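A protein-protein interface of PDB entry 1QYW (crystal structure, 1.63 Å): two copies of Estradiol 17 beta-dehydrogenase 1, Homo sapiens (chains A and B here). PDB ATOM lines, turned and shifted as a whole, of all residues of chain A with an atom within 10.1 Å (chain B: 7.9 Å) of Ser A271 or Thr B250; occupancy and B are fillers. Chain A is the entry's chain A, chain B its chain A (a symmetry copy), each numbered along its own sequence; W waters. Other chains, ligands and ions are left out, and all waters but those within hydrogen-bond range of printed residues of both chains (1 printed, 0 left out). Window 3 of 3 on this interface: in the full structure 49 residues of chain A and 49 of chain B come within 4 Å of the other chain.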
ATOM      1  N   MET A 265     -25.356  12.126 -21.543  1.00  0.00           N
ATOM      2  CA  MET A 265     -24.807  13.243 -20.794  1.00  0.00           C
ATOM      3  C   MET A 265     -25.805  13.674 -19.715  1.00  0.00           C
ATOM      4  O   MET A 265     -25.516  13.921 -18.554  1.00  0.00           O
ATOM      5  CB  MET A 265     -24.595  14.433 -21.720  1.00  0.00           C
ATOM      6  CG  MET A 265     -24.627  15.778 -20.992  1.00  0.00           C
ATOM      7  SD  MET A 265     -23.959  17.092 -22.012  1.00  0.00           S
ATOM      8  CE  MET A 265     -22.306  16.467 -22.323  1.00  0.00           C
ATOM      9  N   ARG A 266     -27.047  13.845 -20.207  1.00  0.00           N
ATOM     10  CA  ARG A 266     -28.114  14.244 -19.298  1.00  0.00           C
ATOM     11  C   ARG A 266     -28.220  13.235 -18.170  1.00  0.00           C
ATOM     12  O   ARG A 266     -28.172  13.534 -16.980  1.00  0.00           O
ATOM     13  CB  ARG A 266     -29.426  14.299 -20.108  1.00  0.00           C
ATOM     14  CG  ARG A 266     -30.595  14.708 -19.245  1.00  0.00           C
ATOM     15  CD  ARG A 266     -31.941  14.514 -19.994  1.00  0.00           C
ATOM     16  NE  ARG A 266     -32.926  15.006 -19.004  1.00  0.00           N
ATOM     17  CZ  ARG A 266     -33.512  14.331 -18.050  1.00  0.00           C
ATOM     18  NH1 ARG A 266     -33.386  13.008 -17.903  1.00  0.00           N
ATOM     19  NH2 ARG A 266     -34.314  15.004 -17.195  1.00  0.00           N
ATOM     20  N   LEU A 267     -28.330  11.952 -18.525  1.00  0.00           N
ATOM     21  CA  LEU A 267     -28.525  10.894 -17.542  1.00  0.00           C
ATOM     22  C   LEU A 267     -27.333  10.687 -16.616  1.00  0.00           C
ATOM     23  O   LEU A 267     -27.515  10.208 -15.494  1.00  0.00           O
ATOM     24  CB  LEU A 267     -28.928   9.585 -18.226  1.00  0.00           C
ATOM     25  CG  LEU A 267     -30.113   9.623 -19.196  1.00  0.00           C
ATOM     26  CD1 LEU A 267     -30.412   8.263 -19.807  1.00  0.00           C
ATOM     27  CD2 LEU A 267     -31.375  10.167 -18.556  1.00  0.00           C
ATOM     28  N   ASP A 268     -26.133  11.051 -17.020  1.00  0.00           N
ATOM     29  CA  ASP A 268     -24.930  10.897 -16.230  1.00  0.00           C
ATOM     30  C   ASP A 268     -24.637  12.005 -15.239  1.00  0.00           C
ATOM     31  O   ASP A 268     -23.657  11.906 -14.475  1.00  0.00           O
ATOM     32  CB  ASP A 268     -23.728  10.792 -17.180  1.00  0.00           C
ATOM     33  CG  ASP A 268     -23.628   9.440 -17.853  1.00  0.00           C
ATOM     34  OD1 ASP A 268     -24.344   8.501 -17.438  1.00  0.00           O
ATOM     35  OD2 ASP A 268     -22.825   9.317 -18.804  1.00  0.00           O
ATOM     36  N   ASP A 269     -25.358  13.119 -15.286  1.00  0.00           N
ATOM     37  CA  ASP A 269     -25.151  14.203 -14.326  1.00  0.00           C
ATOM     38  C   ASP A 269     -26.559  14.577 -13.845  1.00  0.00           C
ATOM     39  O   ASP A 269     -27.205  15.475 -14.377  1.00  0.00           O
ATOM     40  CB  ASP A 269     -24.431  15.435 -14.847  1.00  0.00           C
ATOM     41  CG  ASP A 269     -24.458  16.664 -13.959  1.00  0.00           C
ATOM     42  OD1 ASP A 269     -24.661  16.568 -12.725  1.00  0.00           O
ATOM     43  OD2 ASP A 269     -24.305  17.800 -14.442  1.00  0.00           O
ATOM     44  N   PRO A 270     -27.009  13.872 -12.830  1.00  0.00           N
ATOM     45  CA  PRO A 270     -28.310  14.086 -12.219  1.00  0.00           C
ATOM     46  C   PRO A 270     -28.512  15.481 -11.666  1.00  0.00           C
ATOM     47  O   PRO A 270     -29.682  15.898 -11.660  1.00  0.00           O
ATOM     48  CB  PRO A 270     -28.434  12.982 -11.179  1.00  0.00           C
ATOM     49  CG  PRO A 270     -27.475  11.934 -11.640  1.00  0.00           C
ATOM     50  CD  PRO A 270     -26.301  12.746 -12.153  1.00  0.00           C
ATOM     51  N   SER A 271     -27.505  16.321 -11.435  1.00  0.00           N
ATOM     52  CA  SER A 271     -27.742  17.701 -11.018  1.00  0.00           C
ATOM     53  C   SER A 271     -28.332  18.532 -12.142  1.00  0.00           C
ATOM     54  O   SER A 271     -28.856  19.632 -11.933  1.00  0.00           O
ATOM     55  CB  SER A 271     -26.458  18.382 -10.508  1.00  0.00           C
ATOM     56  OG  SER A 271     -25.637  18.772 -11.619  1.00  0.00           O
ATOM     57  N   GLY A 272     -28.165  18.034 -13.398  1.00  0.00           N
ATOM     58  CA  GLY A 272     -28.683  18.710 -14.571  1.00  0.00           C
ATOM     59  C   GLY A 272     -27.748  19.738 -15.172  1.00  0.00           C
ATOM     60  O   GLY A 272     -28.013  20.238 -16.261  1.00  0.00           O
ATOM     61  N   SER A 273     -26.679  20.135 -14.490  1.00  0.00           N
ATOM     62  CA  SER A 273     -25.748  21.158 -14.925  1.00  0.00           C
ATOM     63  C   SER A 273     -25.158  20.901 -16.298  1.00  0.00           C
ATOM     64  O   SER A 273     -25.139  21.799 -17.158  1.00  0.00           O
ATOM     65  CB  SER A 273     -24.591  21.195 -13.875  1.00  0.00           C
ATOM     66  OG  SER A 273     -23.657  22.209 -14.226  1.00  0.00           O
ATOM     67  N   ASN A 274     -24.638  19.713 -16.503  1.00  0.00           N
ATOM     68  CA  ASN A 274     -24.006  19.415 -17.797  1.00  0.00           C
ATOM     69  C   ASN A 274     -24.992  19.532 -18.957  1.00  0.00           C
ATOM     70  O   ASN A 274     -24.649  20.111 -19.979  1.00  0.00           O
ATOM     71  CB  ASN A 274     -23.358  18.040 -17.766  1.00  0.00           C
ATOM     72  CG  ASN A 274     -22.108  18.063 -16.877  1.00  0.00           C
ATOM     73  OD1 ASN A 274     -21.675  19.112 -16.398  1.00  0.00           O
ATOM     74  ND2 ASN A 274     -21.557  16.871 -16.678  1.00  0.00           N
ATOM     75  N   TYR A 275     -26.184  18.977 -18.777  1.00  0.00           N
ATOM     76  CA  TYR A 275     -27.190  19.025 -19.830  1.00  0.00           C
ATOM     77  C   TYR A 275     -27.596  20.441 -20.147  1.00  0.00           C
ATOM     78  O   TYR A 275     -27.710  20.857 -21.315  1.00  0.00           O
ATOM     79  CB  TYR A 275     -28.401  18.129 -19.471  1.00  0.00           C
ATOM     80  CG  TYR A 275     -29.438  18.309 -20.578  1.00  0.00           C
ATOM     81  CD1 TYR A 275     -29.285  17.637 -21.778  1.00  0.00           C
ATOM     82  CD2 TYR A 275     -30.515  19.174 -20.386  1.00  0.00           C
ATOM     83  CE1 TYR A 275     -30.213  17.810 -22.799  1.00  0.00           C
ATOM     84  CE2 TYR A 275     -31.443  19.363 -21.410  1.00  0.00           C
ATOM     85  CZ  TYR A 275     -31.274  18.669 -22.584  1.00  0.00           C
ATOM     86  OH  TYR A 275     -32.151  18.815 -23.651  1.00  0.00           O
ATOM     87  N   VAL A 276     -27.918  21.226 -19.093  1.00  0.00           N
ATOM     88  CA  VAL A 276     -28.357  22.596 -19.329  1.00  0.00           C
ATOM     89  C   VAL A 276     -27.304  23.404 -20.079  1.00  0.00           C
ATOM     90  O   VAL A 276     -27.641  24.124 -21.018  1.00  0.00           O
ATOM     91  CB  VAL A 276     -28.784  23.248 -18.001  1.00  0.00           C
ATOM     92  CG1 VAL A 276     -29.106  24.709 -18.154  1.00  0.00           C
ATOM     93  CG2 VAL A 276     -30.013  22.457 -17.511  1.00  0.00           C
ATOM     94  N   THR A 277     -26.030  23.313 -19.691  1.00  0.00           N
ATOM     95  CA  THR A 277     -24.981  24.044 -20.395  1.00  0.00           C
ATOM     96  C   THR A 277     -24.829  23.531 -21.828  1.00  0.00           C
ATOM     97  O   THR A 277     -24.803  24.336 -22.766  1.00  0.00           O
ATOM     98  CB  THR A 277     -23.654  23.913 -19.624  1.00  0.00           C
ATOM     99  OG1 THR A 277     -23.853  24.555 -18.339  1.00  0.00           O
ATOM    100  CG2 THR A 277     -22.496  24.574 -20.343  1.00  0.00           C
ATOM    101  N   ARG B 136     -35.239  33.637  -7.756  1.00  0.00           N
ATOM    102  CA  ARG B 136     -35.048  32.212  -7.580  1.00  0.00           C
ATOM    103  C   ARG B 136     -36.417  31.543  -7.613  1.00  0.00           C
ATOM    104  O   ARG B 136     -37.408  32.058  -7.132  1.00  0.00           O
ATOM    105  CB  ARG B 136     -34.344  31.852  -6.287  1.00  0.00           C
ATOM    106  CG  ARG B 136     -32.992  32.464  -6.008  1.00  0.00           C
ATOM    107  CD  ARG B 136     -31.922  32.135  -7.021  1.00  0.00           C
ATOM    108  NE  ARG B 136     -30.681  32.819  -6.639  1.00  0.00           N
ATOM    109  CZ  ARG B 136     -29.717  32.299  -5.896  1.00  0.00           C
ATOM    110  NH1 ARG B 136     -29.740  31.049  -5.446  1.00  0.00           N
ATOM    111  NH2 ARG B 136     -28.670  33.085  -5.637  1.00  0.00           N
ATOM    112  N   VAL B 137     -36.440  30.443  -8.408  1.00  0.00           N
ATOM    113  CA  VAL B 137     -37.667  29.652  -8.456  1.00  0.00           C
ATOM    114  C   VAL B 137     -37.285  28.238  -7.994  1.00  0.00           C
ATOM    115  O   VAL B 137     -36.376  27.633  -8.555  1.00  0.00           O
ATOM    116  CB  VAL B 137     -38.300  29.580  -9.849  1.00  0.00           C
ATOM    117  CG1 VAL B 137     -39.555  28.710  -9.848  1.00  0.00           C
ATOM    118  CG2 VAL B 137     -38.650  30.961 -10.391  1.00  0.00           C
ATOM    119  N   LEU B 138     -37.929  27.762  -6.936  1.00  0.00           N
ATOM    120  CA  LEU B 138     -37.745  26.408  -6.441  1.00  0.00           C
ATOM    121  C   LEU B 138     -39.033  25.624  -6.657  1.00  0.00           C
ATOM    122  O   LEU B 138     -40.132  26.095  -6.332  1.00  0.00           O
ATOM    123  CB  LEU B 138     -37.383  26.349  -4.953  1.00  0.00           C
ATOM    124  CG  LEU B 138     -36.204  27.227  -4.539  1.00  0.00           C
ATOM    125  CD1 LEU B 138     -36.009  27.106  -3.031  1.00  0.00           C
ATOM    126  CD2 LEU B 138     -34.937  26.837  -5.284  1.00  0.00           C
ATOM    127  N   GLU B 167     -36.753  21.773 -16.881  1.00  0.00           N
ATOM    128  CA  GLU B 167     -35.518  21.585 -17.610  1.00  0.00           C
ATOM    129  C   GLU B 167     -35.497  22.437 -18.872  1.00  0.00           C
ATOM    130  O   GLU B 167     -34.546  23.136 -19.197  1.00  0.00           O
ATOM    131  CB  GLU B 167     -35.320  20.102 -17.901  1.00  0.00           C
ATOM    132  CG  GLU B 167     -33.919  19.827 -18.430  1.00  0.00           C
ATOM    133  CD  GLU B 167     -33.706  18.325 -18.400  1.00  0.00           C
ATOM    134  OE1 GLU B 167     -33.793  17.699 -19.464  1.00  0.00           O
ATOM    135  OE2 GLU B 167     -33.464  17.741 -17.318  1.00  0.00           O
ATOM    136  N   ALA B 170     -35.006  26.037 -17.838  1.00  0.00           N
ATOM    137  CA  ALA B 170     -33.633  26.264 -17.384  1.00  0.00           C
ATOM    138  C   ALA B 170     -32.689  26.523 -18.560  1.00  0.00           C
ATOM    139  O   ALA B 170     -31.752  27.307 -18.429  1.00  0.00           O
ATOM    140  CB  ALA B 170     -33.062  25.110 -16.582  1.00  0.00           C
ATOM    141  N   HIS B 179     -32.840  31.861 -11.605  1.00  0.00           N
ATOM    142  CA  HIS B 179     -32.392  30.505 -11.336  1.00  0.00           C
ATOM    143  C   HIS B 179     -33.534  29.596 -10.918  1.00  0.00           C
ATOM    144  O   HIS B 179     -34.254  29.965 -10.005  1.00  0.00           O
ATOM    145  CB  HIS B 179     -31.361  30.578 -10.194  1.00  0.00           C
ATOM    146  CG  HIS B 179     -30.191  31.453 -10.549  1.00  0.00           C
ATOM    147  ND1 HIS B 179     -30.076  32.755 -10.143  1.00  0.00           N
ATOM    148  CD2 HIS B 179     -29.096  31.172 -11.296  1.00  0.00           C
ATOM    149  CE1 HIS B 179     -28.942  33.251 -10.620  1.00  0.00           C
ATOM    150  NE2 HIS B 179     -28.323  32.311 -11.313  1.00  0.00           N
ATOM    151  N   LEU B 180     -33.726  28.533 -11.664  1.00  0.00           N
ATOM    152  CA  LEU B 180     -34.777  27.548 -11.388  1.00  0.00           C
ATOM    153  C   LEU B 180     -34.157  26.248 -10.933  1.00  0.00           C
ATOM    154  O   LEU B 180     -33.202  25.691 -11.492  1.00  0.00           O
ATOM    155  CB  LEU B 180     -35.582  27.305 -12.682  1.00  0.00           C
ATOM    156  CG  LEU B 180     -36.886  26.504 -12.498  1.00  0.00           C
ATOM    157  CD1 LEU B 180     -37.814  26.782 -13.671  1.00  0.00           C
ATOM    158  CD2 LEU B 180     -36.627  25.009 -12.412  1.00  0.00           C
ATOM    159  N   SER B 181     -34.692  25.699  -9.841  1.00  0.00           N
ATOM    160  CA  SER B 181     -34.192  24.451  -9.313  1.00  0.00           C
ATOM    161  C   SER B 181     -35.336  23.552  -8.841  1.00  0.00           C
ATOM    162  O   SER B 181     -36.247  24.074  -8.208  1.00  0.00           O
ATOM    163  CB  SER B 181     -33.301  24.659  -8.084  1.00  0.00           C
ATOM    164  OG  SER B 181     -32.162  25.441  -8.424  1.00  0.00           O
ATOM    165  N   LEU B 182     -35.201  22.274  -9.108  1.00  0.00           N
ATOM    166  CA  LEU B 182     -36.111  21.265  -8.579  1.00  0.00           C
ATOM    167  C   LEU B 182     -35.512  20.637  -7.329  1.00  0.00           C
ATOM    168  O   LEU B 182     -34.297  20.364  -7.279  1.00  0.00           O
ATOM    169  CB  LEU B 182     -36.226  20.099  -9.617  1.00  0.00           C
ATOM    170  CG  LEU B 182     -37.021  20.502 -10.862  1.00  0.00           C
ATOM    171  CD1 LEU B 182     -36.493  19.711 -12.083  1.00  0.00           C
ATOM    172  CD2 LEU B 182     -38.484  20.143 -10.581  1.00  0.00           C
ATOM    173  N   ILE B 183     -36.354  20.509  -6.310  1.00  0.00           N
ATOM    174  CA  ILE B 183     -35.936  19.907  -5.062  1.00  0.00           C
ATOM    175  C   ILE B 183     -36.540  18.508  -5.021  1.00  0.00           C
ATOM    176  O   ILE B 183     -37.752  18.281  -4.894  1.00  0.00           O
ATOM    177  CB  ILE B 183     -36.339  20.704  -3.805  1.00  0.00           C
ATOM    178  CG1 ILE B 183     -35.955  22.164  -3.927  1.00  0.00           C
ATOM    179  CG2 ILE B 183     -35.730  19.969  -2.626  1.00  0.00           C
ATOM    180  CD1 ILE B 183     -34.471  22.474  -4.134  1.00  0.00           C
ATOM    181  N   ALA B 243     -30.499  25.370  -1.518  1.00  0.00           N
ATOM    182  CA  ALA B 243     -30.614  25.801  -2.894  1.00  0.00           C
ATOM    183  C   ALA B 243     -30.765  27.310  -3.043  1.00  0.00           C
ATOM    184  O   ALA B 243     -30.213  27.942  -3.934  1.00  0.00           O
ATOM    185  CB  ALA B 243     -31.822  25.130  -3.578  1.00  0.00           C
ATOM    186  N   ALA B 246     -27.355  29.149  -2.582  1.00  0.00           N
ATOM    187  CA  ALA B 246     -26.259  28.812  -3.487  1.00  0.00           C
ATOM    188  C   ALA B 246     -26.095  29.957  -4.465  1.00  0.00           C
ATOM    189  O   ALA B 246     -27.053  30.461  -5.065  1.00  0.00           O
ATOM    190  CB  ALA B 246     -26.575  27.479  -4.173  1.00  0.00           C
ATOM    191  N   PRO B 247     -24.864  30.428  -4.655  1.00  0.00           N
ATOM    192  CA  PRO B 247     -24.582  31.480  -5.610  1.00  0.00           C
ATOM    193  C   PRO B 247     -24.954  31.094  -7.031  1.00  0.00           C
ATOM    194  O   PRO B 247     -25.515  31.878  -7.806  1.00  0.00           O
ATOM    195  CB  PRO B 247     -23.073  31.718  -5.509  1.00  0.00           C
ATOM    196  CG  PRO B 247     -22.636  31.032  -4.278  1.00  0.00           C
ATOM    197  CD  PRO B 247     -23.637  29.942  -3.985  1.00  0.00           C
ATOM    198  N   LYS B 248     -24.658  29.857  -7.413  1.00  0.00           N
ATOM    199  CA  LYS B 248     -24.925  29.316  -8.744  1.00  0.00           C
ATOM    200  C   LYS B 248     -25.649  27.980  -8.599  1.00  0.00           C
ATOM    201  O   LYS B 248     -25.078  26.878  -8.659  1.00  0.00           O
ATOM    202  CB  LYS B 248     -23.608  29.094  -9.502  1.00  0.00           C
ATOM    203  CG  LYS B 248     -22.790  30.344  -9.766  1.00  0.00           C
ATOM    204  CD  LYS B 248     -21.603  30.119 -10.690  1.00  0.00           C
ATOM    205  CE  LYS B 248     -20.799  31.404 -10.843  1.00  0.00           C
ATOM    206  NZ  LYS B 248     -19.530  31.216 -11.602  1.00  0.00           N
ATOM    207  N   PRO B 249     -26.939  28.058  -8.300  1.00  0.00           N
ATOM    208  CA  PRO B 249     -27.703  26.843  -8.049  1.00  0.00           C
ATOM    209  C   PRO B 249     -27.804  25.943  -9.276  1.00  0.00           C
ATOM    210  O   PRO B 249     -27.856  26.413 -10.410  1.00  0.00           O
ATOM    211  CB  PRO B 249     -29.068  27.335  -7.584  1.00  0.00           C
ATOM    212  CG  PRO B 249     -29.180  28.722  -8.113  1.00  0.00           C
ATOM    213  CD  PRO B 249     -27.778  29.267  -8.196  1.00  0.00           C
ATOM    214  N   THR B 250     -27.773  24.652  -8.996  1.00  0.00           N
ATOM    215  CA  THR B 250     -27.935  23.636 -10.037  1.00  0.00           C
ATOM    216  C   THR B 250     -29.423  23.469 -10.331  1.00  0.00           C
ATOM    217  O   THR B 250     -30.320  23.873  -9.559  1.00  0.00           O
ATOM    218  CB  THR B 250     -27.287  22.302  -9.618  1.00  0.00           C
ATOM    219  OG1 THR B 250     -27.803  21.810  -8.370  1.00  0.00           O
ATOM    220  CG2 THR B 250     -25.780  22.504  -9.441  1.00  0.00           C
ATOM    221  N   LEU B 251     -29.720  22.763 -11.419  1.00  0.00           N
ATOM    222  CA  LEU B 251     -31.129  22.544 -11.772  1.00  0.00           C
ATOM    223  C   LEU B 251     -31.802  21.608 -10.775  1.00  0.00           C
ATOM    224  O   LEU B 251     -33.029  21.712 -10.603  1.00  0.00           O
ATOM    225  CB  LEU B 251     -31.187  21.888 -13.172  1.00  0.00           C
ATOM    226  CG  LEU B 251     -32.556  21.412 -13.636  1.00  0.00           C
ATOM    227  CD1 LEU B 251     -33.517  22.587 -13.694  1.00  0.00           C
ATOM    228  CD2 LEU B 251     -32.481  20.719 -15.012  1.00  0.00           C
ATOM    229  N   ARG B 252     -31.071  20.651 -10.207  1.00  0.00           N
ATOM    230  CA  ARG B 252     -31.679  19.687  -9.307  1.00  0.00           C
ATOM    231  C   ARG B 252     -30.929  19.469  -8.007  1.00  0.00           C
ATOM    232  O   ARG B 252     -29.710  19.287  -8.047  1.00  0.00           O
ATOM    233  CB  ARG B 252     -31.693  18.311  -9.981  1.00  0.00           C
ATOM    234  CG  ARG B 252     -32.909  17.893 -10.679  1.00  0.00           C
ATOM    235  CD  ARG B 252     -32.920  16.448 -11.211  1.00  0.00           C
ATOM    236  NE  ARG B 252     -33.726  16.686 -12.431  1.00  0.00           N
ATOM    237  CZ  ARG B 252     -33.231  17.051 -13.595  1.00  0.00           C
ATOM    238  NH1 ARG B 252     -31.904  17.166 -13.775  1.00  0.00           N
ATOM    239  NH2 ARG B 252     -34.089  17.319 -14.561  1.00  0.00           N
ATOM    240  N   TYR B 253     -31.683  19.432  -6.913  1.00  0.00           N
ATOM    241  CA  TYR B 253     -31.120  19.110  -5.608  1.00  0.00           C
ATOM    242  C   TYR B 253     -31.817  17.812  -5.194  1.00  0.00           C
ATOM    243  O   TYR B 253     -32.957  17.578  -5.642  1.00  0.00           O
ATOM    244  CB  TYR B 253     -31.309  20.177  -4.525  1.00  0.00           C
ATOM    245  CG  TYR B 253     -30.449  21.382  -4.861  1.00  0.00           C
ATOM    246  CD1 TYR B 253     -29.206  21.539  -4.236  1.00  0.00           C
ATOM    247  CD2 TYR B 253     -30.816  22.308  -5.817  1.00  0.00           C
ATOM    248  CE1 TYR B 253     -28.390  22.599  -4.559  1.00  0.00           C
ATOM    249  CE2 TYR B 253     -30.011  23.389  -6.148  1.00  0.00           C
ATOM    250  CZ  TYR B 253     -28.782  23.509  -5.503  1.00  0.00           C
ATOM    251  OH  TYR B 253     -27.985  24.573  -5.857  1.00  0.00           O
ATOM    252  N   PHE B 254     -31.103  16.930  -4.528  1.00  0.00           N
ATOM    253  CA  PHE B 254     -31.697  15.691  -4.031  1.00  0.00           C
ATOM    254  C   PHE B 254     -31.740  15.758  -2.507  1.00  0.00           C
ATOM    255  O   PHE B 254     -30.750  16.100  -1.830  1.00  0.00           O
ATOM    256  CB  PHE B 254     -30.865  14.475  -4.494  1.00  0.00           C
ATOM    257  CG  PHE B 254     -30.956  14.317  -5.996  1.00  0.00           C
ATOM    258  CD1 PHE B 254     -31.941  13.507  -6.541  1.00  0.00           C
ATOM    259  CD2 PHE B 254     -30.064  14.967  -6.819  1.00  0.00           C
ATOM    260  CE1 PHE B 254     -32.018  13.375  -7.939  1.00  0.00           C
ATOM    261  CE2 PHE B 254     -30.139  14.826  -8.199  1.00  0.00           C
ATOM    262  CZ  PHE B 254     -31.127  14.047  -8.739  1.00  0.00           C
ATOM    263  N   LEU B 260     -30.626   7.080  -5.757  1.00  0.00           N
ATOM    264  CA  LEU B 260     -29.675   7.328  -6.833  1.00  0.00           C
ATOM    265  C   LEU B 260     -29.284   6.056  -7.571  1.00  0.00           C
ATOM    266  O   LEU B 260     -29.343   6.021  -8.806  1.00  0.00           O
ATOM    267  CB  LEU B 260     -28.477   8.149  -6.385  1.00  0.00           C
ATOM    268  CG  LEU B 260     -28.734   9.617  -6.024  1.00  0.00           C
ATOM    269  CD1 LEU B 260     -27.412  10.302  -5.702  1.00  0.00           C
ATOM    270  CD2 LEU B 260     -29.469  10.364  -7.129  1.00  0.00           C
ATOM    271  N   LEU B 263     -32.045   5.229  -9.840  1.00  0.00           N
ATOM    272  CA  LEU B 263     -32.025   6.240 -10.887  1.00  0.00           C
ATOM    273  C   LEU B 263     -30.906   5.954 -11.891  1.00  0.00           C
ATOM    274  O   LEU B 263     -31.153   6.084 -13.089  1.00  0.00           O
ATOM    275  CB  LEU B 263     -31.850   7.662 -10.358  1.00  0.00           C
ATOM    276  CG  LEU B 263     -31.737   8.805 -11.361  1.00  0.00           C
ATOM    277  CD1 LEU B 263     -33.078   9.016 -12.065  1.00  0.00           C
ATOM    278  CD2 LEU B 263     -31.308  10.107 -10.709  1.00  0.00           C
HETATM  279  O   HOH W   1     -27.426  22.637 -13.034  1.00  0.00           O
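No position is printed for both chains.
Among the printed residues, pairs that only touch across the chains: Tyr A275 with Glu B167, Arg A266 with Arg B252, Pro A270 with Phe B254, Gly A272 with Arg B252, Val A276 with Ala B170, Ser A271 with Thr B250 and Val A276 with Leu B251.
Printed residues of chain B that touch a printed residue of chain A: Glu B167, Ala B170, Thr B250, Leu B251, Arg B252 and Phe B254.
Hydrophobic or aromatic side chains of chain B that line the printed part of chain A: Leu B251 and Phe B254.
Of the 13 printed residues of chain A, 6 touch a printed residue of chain B.
Hydrophobic or aromatic side chains of chain A within 4 Å of the printed part of chain B: Pro A270, Tyr A275 and Val A276.
Along chain A the printed residues that touch a printed residue of chain B span positions 266 to 276.
Among the printed residues, 11 pairs touch across the chains.
The backbone NH (N) of Leu B182 is in hydrogen-bond range of the backbone carbonyl oxygen (O) of Leu B251 (2.7 Å).
N of Ser A273 lies close to OG of Ser A271, 3.3 Å away.
The side-chain hydroxyl (OG) of Ser B181 lies within hydrogen-bond range of the backbone carbonyl oxygen (O) of Thr B250, at 2.7 Å.
The side-chain carboxylate (OE2) of Glu B167 is in salt-bridge range of the guanidinium group (NH2) of Arg B252 (2.9 Å).
N of Thr B250 lies within hydrogen-bond range of OH of Tyr B253 (3.1 Å).
OD1 of Asp A269 lies within hydrogen-bond range of OG of Ser A271, at 2.7 Å.
The backbone carbonyl oxygen of Pro A270 lies close to the guanidinium group of Arg B252, 3.3 Å away.
The backbone carbonyl oxygen (O) of Ser A271 lies within hydrogen-bond range of the backbone NH (N) of Arg B252, at 3.0 Å.
The backbone carbonyl oxygen of Ser A271 is in hydrogen-bond range of the backbone NH of Leu B251 (3.3 Å).
The guanidinium group of Arg A266 is in salt-bridge range of the side-chain carboxylate of Glu B167 (2.9 Å).
Ser A271 touches three residues of chain B.
Of chain A, only Ser A271 (3.9 Å) comes within 4 Å of Thr B250.
No residue of chain A comes within 4 Å of Pro B249.
Leu B251 touches just these residues of chain A: Ser A271 (3.3 Å) and Val A276 (3.9 Å).
Of the printed residues of chain A, Ala B170 touches Val A276.
Of the printed residues of chain A, Arg B252 touches Arg A266, Pro A270, Ser A271 and Gly A272.
Of the printed residues of chain B, Gly A272 touches Arg B252 (3.7 Å).
Of the printed residues of chain A, Phe B254 touches Pro A270.
Pro B247 touches none of the printed residues of chain A.
The nearest residue of chain A that does not touch Thr B250 is Ser A273 (4.8 Å).
Water W1 bridges N of Leu B251 (2.8 Å) and N of Ser A273 (3.0 Å).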
